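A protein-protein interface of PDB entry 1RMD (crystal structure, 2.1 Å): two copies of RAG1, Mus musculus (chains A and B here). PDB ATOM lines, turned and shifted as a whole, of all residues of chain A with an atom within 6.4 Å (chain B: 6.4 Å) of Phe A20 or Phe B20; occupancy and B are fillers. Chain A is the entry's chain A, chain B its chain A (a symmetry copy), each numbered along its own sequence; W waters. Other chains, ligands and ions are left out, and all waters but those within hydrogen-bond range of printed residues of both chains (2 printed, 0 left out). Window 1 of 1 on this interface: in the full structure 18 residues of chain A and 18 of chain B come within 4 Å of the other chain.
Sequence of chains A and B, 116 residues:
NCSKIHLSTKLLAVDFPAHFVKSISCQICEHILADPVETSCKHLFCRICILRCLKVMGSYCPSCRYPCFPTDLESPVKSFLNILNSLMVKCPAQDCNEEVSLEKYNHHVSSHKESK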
ATOM      1  N   LEU A  12      -2.912 -26.616 -40.358  1.00  0.00           N
ATOM      2  CA  LEU A  12      -2.837 -27.232 -39.029  1.00  0.00           C
ATOM      3  C   LEU A  12      -2.452 -28.692 -39.170  1.00  0.00           C
ATOM      4  O   LEU A  12      -3.065 -29.435 -39.944  1.00  0.00           O
ATOM      5  CB  LEU A  12      -4.188 -27.160 -38.322  1.00  0.00           C
ATOM      6  CG  LEU A  12      -4.587 -25.809 -37.721  1.00  0.00           C
ATOM      7  CD1 LEU A  12      -6.041 -25.836 -37.225  1.00  0.00           C
ATOM      8  CD2 LEU A  12      -3.598 -25.436 -36.611  1.00  0.00           C
ATOM      9  N   PHE A  16      -8.259 -31.329 -35.700  1.00  0.00           N
ATOM     10  CA  PHE A  16      -9.130 -30.978 -34.570  1.00  0.00           C
ATOM     11  C   PHE A  16     -10.637 -30.977 -34.898  1.00  0.00           C
ATOM     12  O   PHE A  16     -11.019 -30.934 -36.078  1.00  0.00           O
ATOM     13  CB  PHE A  16      -8.759 -29.571 -34.075  1.00  0.00           C
ATOM     14  CG  PHE A  16      -7.422 -29.474 -33.376  1.00  0.00           C
ATOM     15  CD1 PHE A  16      -7.183 -30.156 -32.197  1.00  0.00           C
ATOM     16  CD2 PHE A  16      -6.422 -28.654 -33.887  1.00  0.00           C
ATOM     17  CE1 PHE A  16      -5.966 -30.026 -31.523  1.00  0.00           C
ATOM     18  CE2 PHE A  16      -5.201 -28.513 -33.228  1.00  0.00           C
ATOM     19  CZ  PHE A  16      -4.969 -29.202 -32.040  1.00  0.00           C
ATOM     20  N   PRO A  17     -11.518 -31.044 -33.860  1.00  0.00           N
ATOM     21  CA  PRO A  17     -12.991 -31.024 -34.061  1.00  0.00           C
ATOM     22  C   PRO A  17     -13.315 -29.659 -34.683  1.00  0.00           C
ATOM     23  O   PRO A  17     -12.583 -28.690 -34.436  1.00  0.00           O
ATOM     24  CB  PRO A  17     -13.527 -31.120 -32.643  1.00  0.00           C
ATOM     25  CG  PRO A  17     -12.484 -31.991 -31.976  1.00  0.00           C
ATOM     26  CD  PRO A  17     -11.178 -31.396 -32.466  1.00  0.00           C
ATOM     27  N   ALA A  18     -14.379 -29.569 -35.482  1.00  0.00           N
ATOM     28  CA  ALA A  18     -14.692 -28.307 -36.173  1.00  0.00           C
ATOM     29  C   ALA A  18     -14.968 -27.077 -35.306  1.00  0.00           C
ATOM     30  O   ALA A  18     -14.604 -25.946 -35.697  1.00  0.00           O
ATOM     31  CB  ALA A  18     -15.826 -28.486 -37.162  1.00  0.00           C
ATOM     32  N   HIS A  19     -15.606 -27.271 -34.153  1.00  0.00           N
ATOM     33  CA  HIS A  19     -15.904 -26.116 -33.312  1.00  0.00           C
ATOM     34  C   HIS A  19     -14.636 -25.573 -32.674  1.00  0.00           C
ATOM     35  O   HIS A  19     -14.508 -24.365 -32.494  1.00  0.00           O
ATOM     36  CB  HIS A  19     -16.997 -26.421 -32.306  1.00  0.00           C
ATOM     37  CG  HIS A  19     -18.362 -26.613 -32.924  1.00  0.00           C
ATOM     38  ND1 HIS A  19     -18.773 -25.948 -34.062  1.00  0.00           N
ATOM     39  CD2 HIS A  19     -19.405 -27.405 -32.561  1.00  0.00           C
ATOM     40  CE1 HIS A  19     -20.005 -26.322 -34.378  1.00  0.00           C
ATOM     41  NE2 HIS A  19     -20.411 -27.204 -33.480  1.00  0.00           N
ATOM     42  N   PHE A  20     -13.660 -26.442 -32.431  1.00  0.00           N
ATOM     43  CA  PHE A  20     -12.410 -25.982 -31.855  1.00  0.00           C
ATOM     44  C   PHE A  20     -11.636 -25.200 -32.925  1.00  0.00           C
ATOM     45  O   PHE A  20     -11.038 -24.167 -32.630  1.00  0.00           O
ATOM     46  CB  PHE A  20     -11.564 -27.135 -31.316  1.00  0.00           C
ATOM     47  CG  PHE A  20     -10.194 -26.708 -30.850  1.00  0.00           C
ATOM     48  CD1 PHE A  20     -10.031 -26.037 -29.637  1.00  0.00           C
ATOM     49  CD2 PHE A  20      -9.081 -26.930 -31.640  1.00  0.00           C
ATOM     50  CE1 PHE A  20      -8.771 -25.588 -29.219  1.00  0.00           C
ATOM     51  CE2 PHE A  20      -7.815 -26.484 -31.229  1.00  0.00           C
ATOM     52  CZ  PHE A  20      -7.665 -25.811 -30.015  1.00  0.00           C
ATOM     53  N   VAL A  21     -11.641 -25.702 -34.157  1.00  0.00           N
ATOM     54  CA  VAL A  21     -10.955 -25.035 -35.245  1.00  0.00           C
ATOM     55  C   VAL A  21     -11.523 -23.622 -35.418  1.00  0.00           C
ATOM     56  O   VAL A  21     -10.796 -22.644 -35.696  1.00  0.00           O
ATOM     57  CB  VAL A  21     -11.152 -25.773 -36.563  1.00  0.00           C
ATOM     58  CG1 VAL A  21     -10.603 -24.920 -37.724  1.00  0.00           C
ATOM     59  CG2 VAL A  21     -10.426 -27.095 -36.527  1.00  0.00           C
ATOM     60  N   LYS A  22     -12.840 -23.540 -35.272  1.00  0.00           N
ATOM     61  CA  LYS A  22     -13.558 -22.288 -35.399  1.00  0.00           C
ATOM     62  C   LYS A  22     -13.142 -21.299 -34.280  1.00  0.00           C
ATOM     63  O   LYS A  22     -13.009 -20.077 -34.515  1.00  0.00           O
ATOM     64  CB  LYS A  22     -15.049 -22.599 -35.332  1.00  0.00           C
ATOM     65  CG  LYS A  22     -15.962 -21.405 -35.390  1.00  0.00           C
ATOM     66  CD  LYS A  22     -16.698 -21.216 -34.081  1.00  0.00           C
ATOM     67  CE  LYS A  22     -17.661 -20.073 -34.221  1.00  0.00           C
ATOM     68  NZ  LYS A  22     -18.523 -20.360 -35.367  1.00  0.00           N
ATOM     69  N   SER A  23     -12.893 -21.856 -33.086  1.00  0.00           N
ATOM     70  CA  SER A  23     -12.509 -21.073 -31.911  1.00  0.00           C
ATOM     71  C   SER A  23     -11.163 -20.391 -32.057  1.00  0.00           C
ATOM     72  O   SER A  23     -10.943 -19.372 -31.439  1.00  0.00           O
ATOM     73  CB  SER A  23     -12.497 -21.927 -30.643  1.00  0.00           C
ATOM     74  OG  SER A  23     -11.379 -22.803 -30.584  1.00  0.00           O
ATOM     75  N   ILE A  24     -10.249 -20.969 -32.833  1.00  0.00           N
ATOM     76  CA  ILE A  24      -8.948 -20.336 -33.011  1.00  0.00           C
ATOM     77  C   ILE A  24      -8.813 -19.578 -34.336  1.00  0.00           C
ATOM     78  O   ILE A  24      -7.706 -19.174 -34.724  1.00  0.00           O
ATOM     79  CB  ILE A  24      -7.788 -21.344 -32.764  1.00  0.00           C
ATOM     80  CG1 ILE A  24      -7.940 -22.615 -33.642  1.00  0.00           C
ATOM     81  CG2 ILE A  24      -7.814 -21.749 -31.285  1.00  0.00           C
ATOM     82  CD1 ILE A  24      -7.659 -22.415 -35.157  1.00  0.00           C
ATOM     83  N   SER A  25      -9.948 -19.388 -35.016  1.00  0.00           N
ATOM     84  CA  SER A  25     -10.004 -18.666 -36.294  1.00  0.00           C
ATOM     85  C   SER A  25     -10.587 -17.232 -36.172  1.00  0.00           C
ATOM     86  O   SER A  25     -11.383 -16.935 -35.287  1.00  0.00           O
ATOM     87  CB  SER A  25     -10.840 -19.454 -37.315  1.00  0.00           C
ATOM     88  OG  SER A  25     -10.372 -20.784 -37.473  1.00  0.00           O
ATOM     89  N   LEU A  44     -13.625 -13.334 -31.150  1.00  0.00           N
ATOM     90  CA  LEU A  44     -12.262 -13.076 -31.623  1.00  0.00           C
ATOM     91  C   LEU A  44     -12.067 -12.675 -33.096  1.00  0.00           C
ATOM     92  O   LEU A  44     -12.762 -13.172 -33.979  1.00  0.00           O
ATOM     93  CB  LEU A  44     -11.392 -14.294 -31.304  1.00  0.00           C
ATOM     94  CG  LEU A  44     -11.367 -14.716 -29.828  1.00  0.00           C
ATOM     95  CD1 LEU A  44     -10.447 -15.870 -29.633  1.00  0.00           C
ATOM     96  CD2 LEU A  44     -10.934 -13.557 -28.942  1.00  0.00           C
ATOM     97  N   PHE A  80      -5.744 -18.864 -23.194  1.00  0.00           N
ATOM     98  CA  PHE A  80      -6.217 -19.058 -24.561  1.00  0.00           C
ATOM     99  C   PHE A  80      -5.052 -18.787 -25.484  1.00  0.00           C
ATOM    100  O   PHE A  80      -4.796 -19.544 -26.416  1.00  0.00           O
ATOM    101  CB  PHE A  80      -7.363 -18.127 -24.934  1.00  0.00           C
ATOM    102  CG  PHE A  80      -7.807 -18.300 -26.350  1.00  0.00           C
ATOM    103  CD1 PHE A  80      -8.524 -19.433 -26.731  1.00  0.00           C
ATOM    104  CD2 PHE A  80      -7.413 -17.405 -27.330  1.00  0.00           C
ATOM    105  CE1 PHE A  80      -8.832 -19.664 -28.080  1.00  0.00           C
ATOM    106  CE2 PHE A  80      -7.714 -17.629 -28.679  1.00  0.00           C
ATOM    107  CZ  PHE A  80      -8.419 -18.754 -29.051  1.00  0.00           C
ATOM    108  N   ILE A  83      -2.799 -21.802 -25.851  1.00  0.00           N
ATOM    109  CA  ILE A  83      -3.316 -22.882 -26.693  1.00  0.00           C
ATOM    110  C   ILE A  83      -3.118 -22.530 -28.184  1.00  0.00           C
ATOM    111  O   ILE A  83      -2.620 -23.331 -28.995  1.00  0.00           O
ATOM    112  CB  ILE A  83      -4.800 -23.131 -26.361  1.00  0.00           C
ATOM    113  CG1 ILE A  83      -4.909 -23.759 -24.954  1.00  0.00           C
ATOM    114  CG2 ILE A  83      -5.420 -23.997 -27.415  1.00  0.00           C
ATOM    115  CD1 ILE A  83      -6.294 -23.690 -24.284  1.00  0.00           C
ATOM    116  N   LEU A  84      -3.440 -21.287 -28.510  1.00  0.00           N
ATOM    117  CA  LEU A  84      -3.298 -20.764 -29.855  1.00  0.00           C
ATOM    118  C   LEU A  84      -1.832 -20.731 -30.284  1.00  0.00           C
ATOM    119  O   LEU A  84      -1.484 -21.276 -31.319  1.00  0.00           O
ATOM    120  CB  LEU A  84      -3.866 -19.349 -29.906  1.00  0.00           C
ATOM    121  CG  LEU A  84      -3.560 -18.528 -31.154  1.00  0.00           C
ATOM    122  CD1 LEU A  84      -4.470 -18.987 -32.305  1.00  0.00           C
ATOM    123  CD2 LEU A  84      -3.751 -17.025 -30.839  1.00  0.00           C
ATOM    124  N   LEU A  87      -0.309 -24.229 -31.324  1.00  0.00           N
ATOM    125  CA  LEU A  87      -0.828 -25.047 -32.433  1.00  0.00           C
ATOM    126  C   LEU A  87       0.294 -25.478 -33.400  1.00  0.00           C
ATOM    127  O   LEU A  87       1.140 -24.669 -33.790  1.00  0.00           O
ATOM    128  CB  LEU A  87      -1.918 -24.296 -33.236  1.00  0.00           C
ATOM    129  CG  LEU A  87      -3.200 -23.770 -32.596  1.00  0.00           C
ATOM    130  CD1 LEU A  87      -4.109 -23.178 -33.687  1.00  0.00           C
ATOM    131  CD2 LEU A  87      -3.922 -24.885 -31.852  1.00  0.00           C
ATOM    132  N   LEU B  12     -15.624 -23.126 -14.868  1.00  0.00           N
ATOM    133  CA  LEU B  12     -14.295 -22.897 -15.444  1.00  0.00           C
ATOM    134  C   LEU B  12     -13.637 -21.724 -14.744  1.00  0.00           C
ATOM    135  O   LEU B  12     -14.231 -20.648 -14.617  1.00  0.00           O
ATOM    136  CB  LEU B  12     -14.398 -22.568 -16.931  1.00  0.00           C
ATOM    137  CG  LEU B  12     -14.656 -23.738 -17.885  1.00  0.00           C
ATOM    138  CD1 LEU B  12     -14.934 -23.234 -19.309  1.00  0.00           C
ATOM    139  CD2 LEU B  12     -13.472 -24.709 -17.829  1.00  0.00           C
ATOM    140  N   PHE B  16     -12.552 -17.786 -20.746  1.00  0.00           N
ATOM    141  CA  PHE B  16     -12.212 -17.992 -22.162  1.00  0.00           C
ATOM    142  C   PHE B  16     -13.174 -17.314 -23.157  1.00  0.00           C
ATOM    143  O   PHE B  16     -14.298 -16.942 -22.785  1.00  0.00           O
ATOM    144  CB  PHE B  16     -12.218 -19.500 -22.461  1.00  0.00           C
ATOM    145  CG  PHE B  16     -11.082 -20.276 -21.833  1.00  0.00           C
ATOM    146  CD1 PHE B  16      -9.768 -20.022 -22.179  1.00  0.00           C
ATOM    147  CD2 PHE B  16     -11.349 -21.299 -20.928  1.00  0.00           C
ATOM    148  CE1 PHE B  16      -8.722 -20.775 -21.639  1.00  0.00           C
ATOM    149  CE2 PHE B  16     -10.317 -22.060 -20.380  1.00  0.00           C
ATOM    150  CZ  PHE B  16      -8.996 -21.798 -20.735  1.00  0.00           C
ATOM    151  N   PRO B  17     -12.741 -17.123 -24.437  1.00  0.00           N
ATOM    152  CA  PRO B  17     -13.595 -16.502 -25.484  1.00  0.00           C
ATOM    153  C   PRO B  17     -14.786 -17.450 -25.674  1.00  0.00           C
ATOM    154  O   PRO B  17     -14.642 -18.661 -25.451  1.00  0.00           O
ATOM    155  CB  PRO B  17     -12.691 -16.508 -26.705  1.00  0.00           C
ATOM    156  CG  PRO B  17     -11.328 -16.299 -26.080  1.00  0.00           C
ATOM    157  CD  PRO B  17     -11.344 -17.249 -24.898  1.00  0.00           C
ATOM    158  N   ALA B  18     -15.949 -16.928 -26.069  1.00  0.00           N
ATOM    159  CA  ALA B  18     -17.148 -17.774 -26.190  1.00  0.00           C
ATOM    160  C   ALA B  18     -17.091 -18.943 -27.174  1.00  0.00           C
ATOM    161  O   ALA B  18     -17.685 -20.010 -26.906  1.00  0.00           O
ATOM    162  CB  ALA B  18     -18.383 -16.943 -26.472  1.00  0.00           C
ATOM    163  N   HIS B  19     -16.404 -18.763 -28.301  1.00  0.00           N
ATOM    164  CA  HIS B  19     -16.347 -19.851 -29.271  1.00  0.00           C
ATOM    165  C   HIS B  19     -15.472 -20.984 -28.759  1.00  0.00           C
ATOM    166  O   HIS B  19     -15.759 -22.149 -29.025  1.00  0.00           O
ATOM    167  CB  HIS B  19     -15.944 -19.357 -30.647  1.00  0.00           C
ATOM    168  CG  HIS B  19     -16.989 -18.501 -31.322  1.00  0.00           C
ATOM    169  ND1 HIS B  19     -18.345 -18.680 -31.132  1.00  0.00           N
ATOM    170  CD2 HIS B  19     -16.870 -17.454 -32.181  1.00  0.00           C
ATOM    171  CE1 HIS B  19     -19.018 -17.782 -31.837  1.00  0.00           C
ATOM    172  NE2 HIS B  19     -18.145 -17.029 -32.485  1.00  0.00           N
ATOM    173  N   PHE B  20     -14.475 -20.658 -27.944  1.00  0.00           N
ATOM    174  CA  PHE B  20     -13.623 -21.697 -27.393  1.00  0.00           C
ATOM    175  C   PHE B  20     -14.420 -22.472 -26.334  1.00  0.00           C
ATOM    176  O   PHE B  20     -14.326 -23.696 -26.259  1.00  0.00           O
ATOM    177  CB  PHE B  20     -12.339 -21.130 -26.789  1.00  0.00           C
ATOM    178  CG  PHE B  20     -11.505 -22.163 -26.074  1.00  0.00           C
ATOM    179  CD1 PHE B  20     -10.746 -23.089 -26.792  1.00  0.00           C
ATOM    180  CD2 PHE B  20     -11.518 -22.245 -24.693  1.00  0.00           C
ATOM    181  CE1 PHE B  20     -10.010 -24.086 -26.139  1.00  0.00           C
ATOM    182  CE2 PHE B  20     -10.783 -23.241 -24.031  1.00  0.00           C
ATOM    183  CZ  PHE B  20     -10.030 -24.162 -24.760  1.00  0.00           C
ATOM    184  N   VAL B  21     -15.189 -21.757 -25.518  1.00  0.00           N
ATOM    185  CA  VAL B  21     -15.994 -22.391 -24.495  1.00  0.00           C
ATOM    186  C   VAL B  21     -16.965 -23.381 -25.147  1.00  0.00           C
ATOM    187  O   VAL B  21     -17.241 -24.484 -24.626  1.00  0.00           O
ATOM    188  CB  VAL B  21     -16.825 -21.371 -23.728  1.00  0.00           C
ATOM    189  CG1 VAL B  21     -17.827 -22.100 -22.809  1.00  0.00           C
ATOM    190  CG2 VAL B  21     -15.924 -20.496 -22.891  1.00  0.00           C
ATOM    191  N   LYS B  22     -17.499 -22.953 -26.285  1.00  0.00           N
ATOM    192  CA  LYS B  22     -18.440 -23.750 -27.048  1.00  0.00           C
ATOM    193  C   LYS B  22     -17.764 -25.038 -27.582  1.00  0.00           C
ATOM    194  O   LYS B  22     -18.381 -26.128 -27.606  1.00  0.00           O
ATOM    195  CB  LYS B  22     -18.957 -22.885 -28.193  1.00  0.00           C
ATOM    196  CG  LYS B  22     -19.912 -23.566 -29.136  1.00  0.00           C
ATOM    197  CD  LYS B  22     -19.301 -23.720 -30.512  1.00  0.00           C
ATOM    198  CE  LYS B  22     -20.323 -24.317 -31.436  1.00  0.00           C
ATOM    199  NZ  LYS B  22     -21.511 -23.466 -31.391  1.00  0.00           N
ATOM    200  N   SER B  23     -16.484 -24.903 -27.955  1.00  0.00           N
ATOM    201  CA  SER B  23     -15.696 -26.007 -28.501  1.00  0.00           C
ATOM    202  C   SER B  23     -15.458 -27.126 -27.506  1.00  0.00           C
ATOM    203  O   SER B  23     -15.280 -28.255 -27.911  1.00  0.00           O
ATOM    204  CB  SER B  23     -14.348 -25.528 -29.041  1.00  0.00           C
ATOM    205  OG  SER B  23     -13.426 -25.214 -28.005  1.00  0.00           O
ATOM    206  N   ILE B  24     -15.409 -26.813 -26.213  1.00  0.00           N
ATOM    207  CA  ILE B  24     -15.197 -27.862 -25.224  1.00  0.00           C
ATOM    208  C   ILE B  24     -16.482 -28.303 -24.516  1.00  0.00           C
ATOM    209  O   ILE B  24     -16.433 -29.026 -23.508  1.00  0.00           O
ATOM    210  CB  ILE B  24     -14.054 -27.488 -24.236  1.00  0.00           C
ATOM    211  CG1 ILE B  24     -14.301 -26.107 -23.572  1.00  0.00           C
ATOM    212  CG2 ILE B  24     -12.739 -27.438 -25.023  1.00  0.00           C
ATOM    213  CD1 ILE B  24     -15.444 -26.070 -22.519  1.00  0.00           C
ATOM    214  N   SER B  25     -17.624 -27.868 -25.057  1.00  0.00           N
ATOM    215  CA  SER B  25     -18.947 -28.210 -24.519  1.00  0.00           C
ATOM    216  C   SER B  25     -19.701 -29.276 -25.358  1.00  0.00           C
ATOM    217  O   SER B  25     -19.496 -29.410 -26.560  1.00  0.00           O
ATOM    218  CB  SER B  25     -19.822 -26.951 -24.415  1.00  0.00           C
ATOM    219  OG  SER B  25     -19.190 -25.923 -23.668  1.00  0.00           O
ATOM    220  N   LEU B  44     -18.742 -32.601 -31.495  1.00  0.00           N
ATOM    221  CA  LEU B  44     -18.583 -33.279 -30.206  1.00  0.00           C
ATOM    222  C   LEU B  44     -19.812 -33.395 -29.287  1.00  0.00           C
ATOM    223  O   LEU B  44     -20.630 -32.482 -29.216  1.00  0.00           O
ATOM    224  CB  LEU B  44     -17.434 -32.616 -29.441  1.00  0.00           C
ATOM    225  CG  LEU B  44     -16.090 -32.571 -30.184  1.00  0.00           C
ATOM    226  CD1 LEU B  44     -15.041 -31.959 -29.322  1.00  0.00           C
ATOM    227  CD2 LEU B  44     -15.659 -33.968 -30.606  1.00  0.00           C
ATOM    228  N   PHE B  80      -6.571 -32.590 -28.696  1.00  0.00           N
ATOM    229  CA  PHE B  80      -7.789 -31.930 -28.235  1.00  0.00           C
ATOM    230  C   PHE B  80      -8.081 -32.442 -26.844  1.00  0.00           C
ATOM    231  O   PHE B  80      -8.389 -31.670 -25.940  1.00  0.00           O
ATOM    232  CB  PHE B  80      -8.993 -32.215 -29.123  1.00  0.00           C
ATOM    233  CG  PHE B  80     -10.245 -31.575 -28.616  1.00  0.00           C
ATOM    234  CD1 PHE B  80     -10.421 -30.196 -28.715  1.00  0.00           C
ATOM    235  CD2 PHE B  80     -11.194 -32.318 -27.934  1.00  0.00           C
ATOM    236  CE1 PHE B  80     -11.535 -29.574 -28.128  1.00  0.00           C
ATOM    237  CE2 PHE B  80     -12.305 -31.705 -27.342  1.00  0.00           C
ATOM    238  CZ  PHE B  80     -12.473 -30.340 -27.439  1.00  0.00           C
ATOM    239  N   ILE B  83      -6.100 -30.591 -24.206  1.00  0.00           N
ATOM    240  CA  ILE B  83      -6.568 -29.241 -23.892  1.00  0.00           C
ATOM    241  C   ILE B  83      -7.792 -29.311 -22.951  1.00  0.00           C
ATOM    242  O   ILE B  83      -7.874 -28.625 -21.918  1.00  0.00           O
ATOM    243  CB  ILE B  83      -6.899 -28.493 -25.198  1.00  0.00           C
ATOM    244  CG1 ILE B  83      -5.589 -28.195 -25.961  1.00  0.00           C
ATOM    245  CG2 ILE B  83      -7.668 -27.245 -24.890  1.00  0.00           C
ATOM    246  CD1 ILE B  83      -5.737 -27.843 -27.454  1.00  0.00           C
ATOM    247  N   LEU B  84      -8.699 -30.214 -23.286  1.00  0.00           N
ATOM    248  CA  LEU B  84      -9.902 -30.447 -22.509  1.00  0.00           C
ATOM    249  C   LEU B  84      -9.570 -30.974 -21.115  1.00  0.00           C
ATOM    250  O   LEU B  84     -10.001 -30.407 -20.125  1.00  0.00           O
ATOM    251  CB  LEU B  84     -10.779 -31.465 -23.234  1.00  0.00           C
ATOM    252  CG  LEU B  84     -11.950 -32.047 -22.449  1.00  0.00           C
ATOM    253  CD1 LEU B  84     -13.095 -31.022 -22.401  1.00  0.00           C
ATOM    254  CD2 LEU B  84     -12.398 -33.374 -23.107  1.00  0.00           C
ATOM    255  N   LEU B  87      -8.264 -28.255 -18.559  1.00  0.00           N
ATOM    256  CA  LEU B  87      -9.049 -27.078 -18.149  1.00  0.00           C
ATOM    257  C   LEU B  87      -9.111 -26.938 -16.614  1.00  0.00           C
ATOM    258  O   LEU B  87      -9.350 -27.915 -15.898  1.00  0.00           O
ATOM    259  CB  LEU B  87     -10.493 -27.131 -18.705  1.00  0.00           C
ATOM    260  CG  LEU B  87     -10.800 -27.221 -20.197  1.00  0.00           C
ATOM    261  CD1 LEU B  87     -12.323 -27.144 -20.411  1.00  0.00           C
ATOM    262  CD2 LEU B  87     -10.101 -26.099 -20.954  1.00  0.00           C
HETATM  263  O   HOH W   1     -12.881 -18.836 -29.180  1.00  0.00           O
HETATM  264  O   HOH W   2     -14.624 -28.438 -30.857  1.00  0.00           O
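Phe A16 touches Phe B80, and with the chains exchanged Phe A80 touches Phe B16.
His A19 touches Lys B22, and with the chains exchanged Lys A22 touches His B19.
Phe B20 touches its own counterpart, Phe A20.
Ile A83 touches its own counterpart, Ile B83.
Positions printed for both chains: 12, 16, 17, 18, 19, 20, 21, 22, 23, 24, 25, 44, 80, 83, 84 and 87.
Of the 16 pairs that touch across the chains among the printed residues, 16 have their exchanged pair printed and touching as well.
Of the printed residues of chain A, Phe B20 touches Phe A20 (3.6 Å), Ser A23 (3.4 Å) and Ile A83 (3.8 Å).
Printed residues of chain B within 4 Å of Pro A17: Leu B44 (3.7 Å) and Phe B80 (3.97 Å).
Of the printed residues of chain B, Phe A16 touches Phe B80.
Of the printed residues of chain B, His A19 touches Lys B22 (3.4 Å) and Ser B23 (3.6 Å).
Of the printed residues of chain B, Leu A44 touches Pro B17 (3.7 Å).
Leu A87 touches none of the printed residues of chain B.
The nearest printed residue of chain B that does not touch Phe A20 is Phe B80 (4.01 Å).
Hydrophobic or aromatic side chains of chain A within 4 Å of the printed part of chain B: Phe A16, Pro A17, His A19, Phe A20, Leu A44, Phe A80 and Ile A83.
Of the 16 printed residues of chain B, 9 touch a printed residue of chain A.
Printed residues of chain B that touch a printed residue of chain A: Phe B16, Pro B17, His B19, Phe B20, Lys B22, Ser B23, Leu B44, Phe B80 and Ile B83.
Hydrophobic or aromatic side chains of chain B that line the printed part of chain A: Phe B16, Pro B17, His B19, Phe B20, Leu B44, Phe B80 and Ile B83.
Water W1 lies within hydrogen-bond range of N of Phe B20 (2.7 Å) and O of Ser A23 (3.0 Å).
Water W2 bridges the backbone NH (N) of Phe A20 (2.7 Å) and the backbone carbonyl oxygen (O) of Ser B23 (3.0 Å).
O of Phe A20 lies within hydrogen-bond range of OG of Ser A23, at 2.5 Å.
The side-chain hydroxyl (OG) of Ser B23 sits at hydrogen-bond distance from the backbone carbonyl oxygen (O) of Phe B20 (2.5 Å).
N of Phe B80 touches CE1 of Phe A16, at 3.9 Å.
Pro A17 touches Phe B80 (CD to CG, 3.97 Å).
Lys B22 touches His A19.
His A19 touches Ser B23.
Phe A20 touches Phe B20 (CE1 to CE1, 3.6 Å).
C of His B19 touches CB of Ser A23, 3.6 Å away.
CD1 of Leu A44 touches CG of Pro B17 (3.7 Å).
Phe A80 touches Phe B16 (N to CE1, 3.9 Å).
Phe A80 touches Pro B17.
CD1 of Ile A83 touches CG2 of Ile B83 (3.9 Å).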
